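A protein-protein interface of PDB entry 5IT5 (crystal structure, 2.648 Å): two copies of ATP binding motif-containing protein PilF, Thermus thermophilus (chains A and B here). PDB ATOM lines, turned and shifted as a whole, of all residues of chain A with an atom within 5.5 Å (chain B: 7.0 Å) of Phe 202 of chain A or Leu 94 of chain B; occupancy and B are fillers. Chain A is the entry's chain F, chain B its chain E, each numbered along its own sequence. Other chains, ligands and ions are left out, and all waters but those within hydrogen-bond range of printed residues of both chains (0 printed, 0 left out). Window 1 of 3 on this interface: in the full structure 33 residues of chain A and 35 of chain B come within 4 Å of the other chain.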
ATOM      1  N   GLN A 169      -8.298 -17.112   3.195  1.00  0.00           N
ATOM      2  CA  GLN A 169      -9.443 -17.521   4.010  1.00  0.00           C
ATOM      3  C   GLN A 169      -9.061 -17.370   5.468  1.00  0.00           C
ATOM      4  O   GLN A 169      -7.945 -17.697   5.873  1.00  0.00           O
ATOM      5  CB  GLN A 169      -9.850 -18.965   3.706  1.00  0.00           C
ATOM      6  CG  GLN A 169     -10.982 -19.499   4.539  1.00  0.00           C
ATOM      7  CD  GLN A 169     -12.293 -18.806   4.251  1.00  0.00           C
ATOM      8  OE1 GLN A 169     -12.794 -18.856   3.128  1.00  0.00           O
ATOM      9  NE2 GLN A 169     -12.864 -18.160   5.267  1.00  0.00           N
ATOM     10  N   THR A 170     -10.007 -16.890   6.255  1.00  0.00           N
ATOM     11  CA  THR A 170      -9.758 -16.438   7.609  1.00  0.00           C
ATOM     12  C   THR A 170     -10.800 -17.036   8.568  1.00  0.00           C
ATOM     13  O   THR A 170     -11.968 -17.222   8.195  1.00  0.00           O
ATOM     14  CB  THR A 170      -9.765 -14.882   7.646  1.00  0.00           C
ATOM     15  OG1 THR A 170      -8.424 -14.382   7.578  1.00  0.00           O
ATOM     16  CG2 THR A 170     -10.394 -14.360   8.870  1.00  0.00           C
ATOM     17  N   ILE A 171     -10.361 -17.371   9.786  1.00  0.00           N
ATOM     18  CA  ILE A 171     -11.265 -17.713  10.881  1.00  0.00           C
ATOM     19  C   ILE A 171     -10.975 -16.757  12.050  1.00  0.00           C
ATOM     20  O   ILE A 171      -9.829 -16.624  12.507  1.00  0.00           O
ATOM     21  CB  ILE A 171     -11.133 -19.212  11.290  1.00  0.00           C
ATOM     22  CG1 ILE A 171     -12.218 -19.585  12.292  1.00  0.00           C
ATOM     23  CG2 ILE A 171      -9.696 -19.568  11.753  1.00  0.00           C
ATOM     24  CD1 ILE A 171     -13.603 -19.358  11.768  1.00  0.00           C
ATOM     25  N   THR A 185     -14.600 -15.847   7.811  1.00  0.00           N
ATOM     26  CA  THR A 185     -15.579 -16.679   8.510  1.00  0.00           C
ATOM     27  C   THR A 185     -15.525 -16.391   9.999  1.00  0.00           C
ATOM     28  O   THR A 185     -14.435 -16.287  10.576  1.00  0.00           O
ATOM     29  CB  THR A 185     -15.322 -18.179   8.248  1.00  0.00           C
ATOM     30  OG1 THR A 185     -15.698 -18.462   6.901  1.00  0.00           O
ATOM     31  CG2 THR A 185     -16.132 -19.093   9.178  1.00  0.00           C
ATOM     32  N   ALA A 198     -13.937 -25.051  11.666  1.00  0.00           N
ATOM     33  CA  ALA A 198     -13.817 -24.260  10.467  1.00  0.00           C
ATOM     34  C   ALA A 198     -12.490 -24.572   9.794  1.00  0.00           C
ATOM     35  O   ALA A 198     -12.391 -24.603   8.567  1.00  0.00           O
ATOM     36  CB  ALA A 198     -13.924 -22.807  10.791  1.00  0.00           C
ATOM     37  N   LEU A 199     -11.467 -24.817  10.607  1.00  0.00           N
ATOM     38  CA  LEU A 199     -10.155 -25.122  10.058  1.00  0.00           C
ATOM     39  C   LEU A 199     -10.208 -26.373   9.182  1.00  0.00           C
ATOM     40  O   LEU A 199      -9.694 -26.367   8.064  1.00  0.00           O
ATOM     41  CB  LEU A 199      -9.126 -25.287  11.174  1.00  0.00           C
ATOM     42  CG  LEU A 199      -7.878 -24.446  10.903  1.00  0.00           C
ATOM     43  CD1 LEU A 199      -8.315 -23.054  10.446  1.00  0.00           C
ATOM     44  CD2 LEU A 199      -6.971 -24.372  12.132  1.00  0.00           C
ATOM     45  N   ARG A 200     -10.853 -27.428   9.680  1.00  0.00           N
ATOM     46  CA  ARG A 200     -11.030 -28.654   8.905  1.00  0.00           C
ATOM     47  C   ARG A 200     -11.740 -28.380   7.597  1.00  0.00           C
ATOM     48  O   ARG A 200     -11.438 -29.006   6.594  1.00  0.00           O
ATOM     49  CB  ARG A 200     -11.806 -29.719   9.703  1.00  0.00           C
ATOM     50  CG  ARG A 200     -10.928 -30.486  10.652  1.00  0.00           C
ATOM     51  CD  ARG A 200     -11.674 -31.518  11.452  1.00  0.00           C
ATOM     52  NE  ARG A 200     -11.597 -31.229  12.885  1.00  0.00           N
ATOM     53  CZ  ARG A 200     -12.604 -30.718  13.597  1.00  0.00           C
ATOM     54  NH1 ARG A 200     -13.778 -30.456  13.017  1.00  0.00           N
ATOM     55  NH2 ARG A 200     -12.444 -30.476  14.893  1.00  0.00           N
ATOM     56  N   ALA A 201     -12.683 -27.444   7.610  1.00  0.00           N
ATOM     57  CA  ALA A 201     -13.440 -27.125   6.411  1.00  0.00           C
ATOM     58  C   ALA A 201     -12.552 -26.387   5.407  1.00  0.00           C
ATOM     59  O   ALA A 201     -12.659 -26.610   4.203  1.00  0.00           O
ATOM     60  CB  ALA A 201     -14.657 -26.304   6.759  1.00  0.00           C
ATOM     61  N   PHE A 202     -11.657 -25.535   5.907  1.00  0.00           N
ATOM     62  CA  PHE A 202     -10.778 -24.752   5.043  1.00  0.00           C
ATOM     63  C   PHE A 202      -9.915 -25.638   4.157  1.00  0.00           C
ATOM     64  O   PHE A 202      -9.566 -25.252   3.039  1.00  0.00           O
ATOM     65  CB  PHE A 202      -9.876 -23.826   5.865  1.00  0.00           C
ATOM     66  CG  PHE A 202     -10.608 -22.682   6.527  1.00  0.00           C
ATOM     67  CD1 PHE A 202     -11.973 -22.510   6.338  1.00  0.00           C
ATOM     68  CD2 PHE A 202      -9.930 -21.779   7.326  1.00  0.00           C
ATOM     69  CE1 PHE A 202     -12.658 -21.488   6.933  1.00  0.00           C
ATOM     70  CE2 PHE A 202     -10.609 -20.721   7.933  1.00  0.00           C
ATOM     71  CZ  PHE A 202     -11.977 -20.580   7.737  1.00  0.00           C
ATOM     72  N   LEU A 203      -9.581 -26.830   4.648  1.00  0.00           N
ATOM     73  CA  LEU A 203      -8.739 -27.747   3.890  1.00  0.00           C
ATOM     74  C   LEU A 203      -9.525 -28.299   2.679  1.00  0.00           C
ATOM     75  O   LEU A 203      -8.951 -28.758   1.685  1.00  0.00           O
ATOM     76  CB  LEU A 203      -8.237 -28.875   4.800  1.00  0.00           C
ATOM     77  CG  LEU A 203      -7.484 -28.543   6.098  1.00  0.00           C
ATOM     78  CD1 LEU A 203      -7.251 -29.794   6.938  1.00  0.00           C
ATOM     79  CD2 LEU A 203      -6.153 -27.886   5.787  1.00  0.00           C
ATOM     80  N   ARG A 204     -10.849 -28.219   2.766  1.00  0.00           N
ATOM     81  CA  ARG A 204     -11.732 -28.635   1.679  1.00  0.00           C
ATOM     82  C   ARG A 204     -12.075 -27.471   0.756  1.00  0.00           C
ATOM     83  O   ARG A 204     -12.930 -27.606  -0.107  1.00  0.00           O
ATOM     84  CB  ARG A 204     -13.029 -29.242   2.248  1.00  0.00           C
ATOM     85  CG  ARG A 204     -12.809 -30.450   3.166  1.00  0.00           C
ATOM     86  CD  ARG A 204     -14.126 -30.970   3.765  1.00  0.00           C
ATOM     87  NE  ARG A 204     -14.108 -30.947   5.239  1.00  0.00           N
ATOM     88  CZ  ARG A 204     -14.940 -30.233   6.014  1.00  0.00           C
ATOM     89  NH1 ARG A 204     -15.899 -29.479   5.477  1.00  0.00           N
ATOM     90  NH2 ARG A 204     -14.829 -30.280   7.338  1.00  0.00           N
ATOM     91  N   GLN A 205     -11.412 -26.334   0.948  1.00  0.00           N
ATOM     92  CA  GLN A 205     -11.849 -25.049   0.375  1.00  0.00           C
ATOM     93  C   GLN A 205     -10.764 -24.457  -0.569  1.00  0.00           C
ATOM     94  O   GLN A 205     -10.794 -23.278  -0.942  1.00  0.00           O
ATOM     95  CB  GLN A 205     -12.205 -24.080   1.531  1.00  0.00           C
ATOM     96  CG  GLN A 205     -13.229 -22.945   1.240  1.00  0.00           C
ATOM     97  CD  GLN A 205     -14.659 -23.391   1.235  1.00  0.00           C
ATOM     98  OE1 GLN A 205     -14.990 -24.438   1.763  1.00  0.00           O
ATOM     99  NE2 GLN A 205     -15.523 -22.594   0.644  1.00  0.00           N
ATOM    100  N   ASP A 206      -9.826 -25.317  -0.965  1.00  0.00           N
ATOM    101  CA  ASP A 206      -8.728 -24.973  -1.868  1.00  0.00           C
ATOM    102  C   ASP A 206      -8.016 -23.713  -1.426  1.00  0.00           C
ATOM    103  O   ASP A 206      -7.900 -22.776  -2.201  1.00  0.00           O
ATOM    104  CB  ASP A 206      -9.253 -24.813  -3.296  1.00  0.00           C
ATOM    105  CG  ASP A 206      -8.137 -24.647  -4.331  1.00  0.00           C
ATOM    106  OD1 ASP A 206      -7.045 -25.221  -4.156  1.00  0.00           O
ATOM    107  OD2 ASP A 206      -8.361 -23.937  -5.332  1.00  0.00           O
ATOM    108  N   PRO A 207      -7.524 -23.686  -0.179  1.00  0.00           N
ATOM    109  CA  PRO A 207      -6.940 -22.438   0.332  1.00  0.00           C
ATOM    110  C   PRO A 207      -5.504 -22.212  -0.135  1.00  0.00           C
ATOM    111  O   PRO A 207      -4.825 -23.190  -0.476  1.00  0.00           O
ATOM    112  CB  PRO A 207      -6.973 -22.648   1.843  1.00  0.00           C
ATOM    113  CG  PRO A 207      -6.653 -24.142   1.977  1.00  0.00           C
ATOM    114  CD  PRO A 207      -7.335 -24.803   0.771  1.00  0.00           C
ATOM    115  N   ILE A 210      -4.101 -19.051   4.889  1.00  0.00           N
ATOM    116  CA  ILE A 210      -5.062 -19.191   5.972  1.00  0.00           C
ATOM    117  C   ILE A 210      -4.611 -18.393   7.182  1.00  0.00           C
ATOM    118  O   ILE A 210      -3.428 -18.452   7.550  1.00  0.00           O
ATOM    119  CB  ILE A 210      -5.244 -20.677   6.361  1.00  0.00           C
ATOM    120  CG1 ILE A 210      -6.251 -21.333   5.443  1.00  0.00           C
ATOM    121  CG2 ILE A 210      -5.754 -20.841   7.770  1.00  0.00           C
ATOM    122  CD1 ILE A 210      -6.090 -22.792   5.430  1.00  0.00           C
ATOM    123  N   MET A 211      -5.531 -17.644   7.800  1.00  0.00           N
ATOM    124  CA  MET A 211      -5.244 -17.053   9.104  1.00  0.00           C
ATOM    125  C   MET A 211      -6.059 -17.706  10.207  1.00  0.00           C
ATOM    126  O   MET A 211      -7.284 -17.801  10.078  1.00  0.00           O
ATOM    127  CB  MET A 211      -5.526 -15.545   9.130  1.00  0.00           C
ATOM    128  CG  MET A 211      -5.245 -14.963  10.526  1.00  0.00           C
ATOM    129  SD  MET A 211      -6.499 -13.866  11.104  1.00  0.00           S
ATOM    130  CE  MET A 211      -5.744 -13.346  12.633  1.00  0.00           C
ATOM    131  N   PRO B  26     -19.206 -14.961  -2.135  1.00  0.00           N
ATOM    132  CA  PRO B  26     -19.962 -13.731  -1.886  1.00  0.00           C
ATOM    133  C   PRO B  26     -19.020 -12.619  -1.435  1.00  0.00           C
ATOM    134  O   PRO B  26     -18.033 -12.860  -0.743  1.00  0.00           O
ATOM    135  CB  PRO B  26     -20.944 -14.131  -0.781  1.00  0.00           C
ATOM    136  CG  PRO B  26     -20.264 -15.270  -0.073  1.00  0.00           C
ATOM    137  CD  PRO B  26     -19.499 -16.011  -1.143  1.00  0.00           C
ATOM    138  N   LYS B  70     -27.090 -23.201   7.087  1.00  0.00           N
ATOM    139  CA  LYS B  70     -26.254 -22.147   6.563  1.00  0.00           C
ATOM    140  C   LYS B  70     -25.190 -21.730   7.587  1.00  0.00           C
ATOM    141  O   LYS B  70     -24.201 -21.094   7.228  1.00  0.00           O
ATOM    142  CB  LYS B  70     -27.120 -20.956   6.131  1.00  0.00           C
ATOM    143  CG  LYS B  70     -28.078 -21.272   4.978  1.00  0.00           C
ATOM    144  CD  LYS B  70     -28.777 -20.024   4.443  1.00  0.00           C
ATOM    145  CE  LYS B  70     -29.567 -20.290   3.145  1.00  0.00           C
ATOM    146  NZ  LYS B  70     -30.583 -21.393   3.281  1.00  0.00           N
ATOM    147  N   ARG B  71     -25.359 -22.117   8.849  1.00  0.00           N
ATOM    148  CA  ARG B  71     -24.383 -21.726   9.860  1.00  0.00           C
ATOM    149  C   ARG B  71     -23.141 -22.633   9.900  1.00  0.00           C
ATOM    150  O   ARG B  71     -22.159 -22.304  10.580  1.00  0.00           O
ATOM    151  CB  ARG B  71     -25.014 -21.704  11.261  1.00  0.00           C
ATOM    152  CG  ARG B  71     -26.304 -20.920  11.430  1.00  0.00           C
ATOM    153  CD  ARG B  71     -27.265 -21.759  12.275  1.00  0.00           C
ATOM    154  NE  ARG B  71     -27.496 -23.071  11.658  1.00  0.00           N
ATOM    155  CZ  ARG B  71     -28.259 -24.031  12.181  1.00  0.00           C
ATOM    156  NH1 ARG B  71     -28.878 -23.831  13.340  1.00  0.00           N
ATOM    157  NH2 ARG B  71     -28.414 -25.186  11.538  1.00  0.00           N
ATOM    158  N   LEU B  72     -23.182 -23.764   9.192  1.00  0.00           N
ATOM    159  CA  LEU B  72     -22.115 -24.766   9.277  1.00  0.00           C
ATOM    160  C   LEU B  72     -21.539 -25.163   7.909  1.00  0.00           C
ATOM    161  O   LEU B  72     -22.225 -25.081   6.894  1.00  0.00           O
ATOM    162  CB  LEU B  72     -22.629 -26.031   9.996  1.00  0.00           C
ATOM    163  CG  LEU B  72     -23.010 -26.025  11.484  1.00  0.00           C
ATOM    164  CD1 LEU B  72     -23.551 -27.383  11.896  1.00  0.00           C
ATOM    165  CD2 LEU B  72     -21.820 -25.626  12.356  1.00  0.00           C
ATOM    166  N   PRO B  73     -20.270 -25.610   7.884  1.00  0.00           N
ATOM    167  CA  PRO B  73     -19.687 -26.096   6.635  1.00  0.00           C
ATOM    168  C   PRO B  73     -20.285 -27.430   6.278  1.00  0.00           C
ATOM    169  O   PRO B  73     -20.699 -28.127   7.188  1.00  0.00           O
ATOM    170  CB  PRO B  73     -18.193 -26.249   6.968  1.00  0.00           C
ATOM    171  CG  PRO B  73     -17.986 -25.529   8.238  1.00  0.00           C
ATOM    172  CD  PRO B  73     -19.289 -25.664   8.979  1.00  0.00           C
ATOM    173  N   GLN B  74     -20.330 -27.777   4.994  1.00  0.00           N
ATOM    174  CA  GLN B  74     -20.766 -29.098   4.553  1.00  0.00           C
ATOM    175  C   GLN B  74     -19.850 -29.517   3.428  1.00  0.00           C
ATOM    176  O   GLN B  74     -19.369 -28.670   2.683  1.00  0.00           O
ATOM    177  CB  GLN B  74     -22.228 -29.092   4.086  1.00  0.00           C
ATOM    178  CG  GLN B  74     -23.234 -28.643   5.147  1.00  0.00           C
ATOM    179  CD  GLN B  74     -24.661 -28.517   4.618  1.00  0.00           C
ATOM    180  OE1 GLN B  74     -25.298 -29.512   4.250  1.00  0.00           O
ATOM    181  NE2 GLN B  74     -25.168 -27.289   4.576  1.00  0.00           N
ATOM    182  N   SER B  92     -17.649 -28.228  -1.423  1.00  0.00           N
ATOM    183  CA  SER B  92     -17.472 -27.656  -0.102  1.00  0.00           C
ATOM    184  C   SER B  92     -18.295 -26.384   0.011  1.00  0.00           C
ATOM    185  O   SER B  92     -18.307 -25.565  -0.892  1.00  0.00           O
ATOM    186  CB  SER B  92     -15.996 -27.380   0.159  1.00  0.00           C
ATOM    187  OG  SER B  92     -15.761 -26.966   1.495  1.00  0.00           O
ATOM    188  N   THR B  93     -19.015 -26.235   1.107  1.00  0.00           N
ATOM    189  CA  THR B  93     -19.715 -24.987   1.383  1.00  0.00           C
ATOM    190  C   THR B  93     -19.271 -24.423   2.726  1.00  0.00           C
ATOM    191  O   THR B  93     -19.068 -25.166   3.691  1.00  0.00           O
ATOM    192  CB  THR B  93     -21.228 -25.169   1.403  1.00  0.00           C
ATOM    193  OG1 THR B  93     -21.553 -26.311   2.216  1.00  0.00           O
ATOM    194  CG2 THR B  93     -21.748 -25.352  -0.018  1.00  0.00           C
ATOM    195  N   LEU B  94     -19.137 -23.109   2.797  1.00  0.00           N
ATOM    196  CA  LEU B  94     -18.571 -22.496   3.973  1.00  0.00           C
ATOM    197  C   LEU B  94     -19.334 -21.245   4.318  1.00  0.00           C
ATOM    198  O   LEU B  94     -19.478 -20.372   3.467  1.00  0.00           O
ATOM    199  CB  LEU B  94     -17.100 -22.160   3.742  1.00  0.00           C
ATOM    200  CG  LEU B  94     -16.435 -21.488   4.940  1.00  0.00           C
ATOM    201  CD1 LEU B  94     -16.210 -22.496   6.088  1.00  0.00           C
ATOM    202  CD2 LEU B  94     -15.143 -20.822   4.513  1.00  0.00           C
ATOM    203  N   PRO B  95     -19.822 -21.146   5.564  1.00  0.00           N
ATOM    204  CA  PRO B  95     -20.372 -19.874   6.038  1.00  0.00           C
ATOM    205  C   PRO B  95     -19.311 -18.772   6.000  1.00  0.00           C
ATOM    206  O   PRO B  95     -18.264 -18.935   6.620  1.00  0.00           O
ATOM    207  CB  PRO B  95     -20.801 -20.178   7.479  1.00  0.00           C
ATOM    208  CG  PRO B  95     -20.134 -21.458   7.828  1.00  0.00           C
ATOM    209  CD  PRO B  95     -19.952 -22.216   6.563  1.00  0.00           C
ATOM    210  N   THR B  96     -19.576 -17.698   5.257  1.00  0.00           N
ATOM    211  CA  THR B  96     -18.689 -16.533   5.161  1.00  0.00           C
ATOM    212  C   THR B  96     -19.446 -15.290   5.615  1.00  0.00           C
ATOM    213  O   THR B  96     -20.666 -15.217   5.468  1.00  0.00           O
ATOM    214  CB  THR B  96     -18.162 -16.340   3.701  1.00  0.00           C
ATOM    215  OG1 THR B  96     -16.899 -17.007   3.540  1.00  0.00           O
ATOM    216  CG2 THR B  96     -18.026 -14.867   3.316  1.00  0.00           C
ATOM    217  N   VAL B  97     -18.728 -14.328   6.185  1.00  0.00           N
ATOM    218  CA  VAL B  97     -19.283 -13.027   6.574  1.00  0.00           C
ATOM    219  C   VAL B  97     -20.258 -12.396   5.549  1.00  0.00           C
ATOM    220  O   VAL B  97     -21.138 -11.607   5.920  1.00  0.00           O
ATOM    221  CB  VAL B  97     -18.112 -12.036   6.882  1.00  0.00           C
ATOM    222  CG1 VAL B  97     -18.453 -10.600   6.508  1.00  0.00           C
ATOM    223  CG2 VAL B  97     -17.671 -12.163   8.367  1.00  0.00           C
ATOM    224  N   GLY B  99     -22.188 -14.366   3.451  1.00  0.00           N
ATOM    225  CA  GLY B  99     -23.052 -15.427   2.972  1.00  0.00           C
ATOM    226  C   GLY B  99     -22.273 -16.694   2.724  1.00  0.00           C
ATOM    227  O   GLY B  99     -21.112 -16.786   3.088  1.00  0.00           O
ATOM    228  N   GLU B 100     -22.903 -17.679   2.099  1.00  0.00           N
ATOM    229  CA  GLU B 100     -22.258 -18.975   1.907  1.00  0.00           C
ATOM    230  C   GLU B 100     -21.368 -19.041   0.648  1.00  0.00           C
ATOM    231  O   GLU B 100     -21.813 -18.772  -0.466  1.00  0.00           O
ATOM    232  CB  GLU B 100     -23.319 -20.071   1.857  1.00  0.00           C
ATOM    233  CG  GLU B 100     -23.294 -20.984   3.055  1.00  0.00           C
ATOM    234  CD  GLU B 100     -24.493 -21.913   3.089  1.00  0.00           C
ATOM    235  OE1 GLU B 100     -24.299 -23.141   3.222  1.00  0.00           O
ATOM    236  OE2 GLU B 100     -25.633 -21.412   2.963  1.00  0.00           O
ATOM    237  N   LYS B 101     -20.105 -19.398   0.858  1.00  0.00           N
ATOM    238  CA  LYS B 101     -19.150 -19.626  -0.213  1.00  0.00           C
ATOM    239  C   LYS B 101     -19.078 -21.107  -0.606  1.00  0.00           C
ATOM    240  O   LYS B 101     -19.030 -21.989   0.249  1.00  0.00           O
ATOM    241  CB  LYS B 101     -17.761 -19.147   0.196  1.00  0.00           C
ATOM    242  CG  LYS B 101     -16.727 -19.407  -0.867  1.00  0.00           C
ATOM    243  CD  LYS B 101     -15.307 -19.311  -0.372  1.00  0.00           C
ATOM    244  CE  LYS B 101     -14.339 -19.376  -1.561  1.00  0.00           C
ATOM    245  NZ  LYS B 101     -12.930 -19.596  -1.149  1.00  0.00           N
ATOM    246  N   ALA B 102     -19.054 -21.386  -1.900  1.00  0.00           N
ATOM    247  CA  ALA B 102     -18.949 -22.770  -2.355  1.00  0.00           C
ATOM    248  C   ALA B 102     -17.632 -23.001  -3.120  1.00  0.00           C
ATOM    249  O   ALA B 102     -17.168 -22.138  -3.869  1.00  0.00           O
ATOM    250  CB  ALA B 102     -20.165 -23.145  -3.220  1.00  0.00           C
ATOM    251  N   VAL B 103     -17.012 -24.151  -2.894  1.00  0.00           N
ATOM    252  CA  VAL B 103     -15.847 -24.542  -3.672  1.00  0.00           C
ATOM    253  C   VAL B 103     -16.028 -25.962  -4.215  1.00  0.00           C
ATOM    254  O   VAL B 103     -16.379 -26.883  -3.478  1.00  0.00           O
ATOM    255  CB  VAL B 103     -14.549 -24.460  -2.838  1.00  0.00           C
ATOM    256  CG1 VAL B 103     -13.387 -25.136  -3.573  1.00  0.00           C
ATOM    257  CG2 VAL B 103     -14.232 -23.002  -2.490  1.00  0.00           C
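The side-chain hydroxyl of Thr 185 of chain A sits at hydrogen-bond distance from the backbone carbonyl oxygen of Pro 95 of chain B (2.6 Å).
OG of Ser 92 of chain B lies within hydrogen-bond range of OE1 of Gln 205 of chain A (2.7 Å).
The backbone carbonyl oxygen (O) of Arg 204 of chain A sits close to the side-chain hydroxyl (OG) of Ser 92 of chain B, 3.3 Å away.
The side-chain hydroxyl (OG1) of Thr 185 of chain A sits at hydrogen-bond distance from the side-chain amide nitrogen (NE2) of Gln 169 of chain A, at 3.3 Å.
The backbone carbonyl oxygen (O) of Thr 170 of chain A lies within hydrogen-bond range of the backbone NH (N) of Thr 185 of chain A (3.0 Å).
The backbone NH (N) of Ser 92 of chain B sits at hydrogen-bond distance from the backbone carbonyl oxygen (O) of Val 103 of chain B (2.8 Å).
The backbone carbonyl oxygen (O) of Gln 169 of chain A is in hydrogen-bond range of the backbone NH (N) of Met 211 of chain A (3.1 Å).
The backbone carbonyl oxygen (O) of Lys 101 of chain B lies within hydrogen-bond range of the backbone NH (N) of Leu 94 of chain B.
Among the printed residues, merely in contact across the chains: Gln 169 of chain A with Leu 94 of chain B (3.4 Å), Thr 185 of chain A with Leu 94 of chain B (3.4 Å), Thr 185 of chain A with Thr 96 of chain B (3.9 Å), Ala 201 of chain A with Pro 73 of chain B (3.5 Å), Phe 202 of chain A with Leu 94 of chain B (3.5 Å), Gln 205 of chain A with Leu 94 of chain B (3.5 Å), Gln 205 of chain A with Lys 101 of chain B (3.4 Å) and Gln 205 of chain A with Val 103 of chain B (3.4 Å).
Of the printed residues of chain B, Gln 169 of chain A touches Leu 94 (3.4 Å).
Printed residues of chain B within 4 Å of Thr 185 of chain A: Leu 94, Pro 95 and Thr 96.
Phe 202 of chain A touches just one residue of chain B: Leu 94.
Printed residues of chain B within 4 Å of Gln 205 of chain A: Ser 92 (2.7 Å), Leu 94 (3.5 Å), Lys 101 (3.4 Å) and Val 103 (3.4 Å).
Of the printed residues of chain A, Ser 92 of chain B touches Arg 204 (3.1 Å) and Gln 205 (2.7 Å).
Leu 94 of chain B touches just these residues of chain A: Gln 169, Thr 185, Phe 202 and Gln 205.
Printed residues of chain A within 4 Å of Thr 96 of chain B: Thr 185 (3.9 Å).
The nearest printed residue of chain B that does not touch Phe 202 of chain A is Pro 95 of chain B (6.2 Å).
The nearest printed residue of chain B that does not touch Thr 185 of chain A is Val 97 of chain B (4.6 Å).
Of the 17 printed residues of chain B, 7 touch a printed residue of chain A.
Hydrophobic or aromatic side chains of chain B within 4 Å of the printed part of chain A: Pro 73, Leu 94 and Val 103.
Hydrophobic or aromatic side chains of chain A that line the printed part of chain B: Ala 201 and Phe 202.
Along chain A the printed residues that touch a printed residue of chain B span positions 169 to 205.
Among the printed residues, 11 pairs touch across the chains.
Among the printed residues, no Asp or Glu carboxylate lies within 4 Å of a Lys or Arg side-chain nitrogen of the other chain.
No position is printed for both chains.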
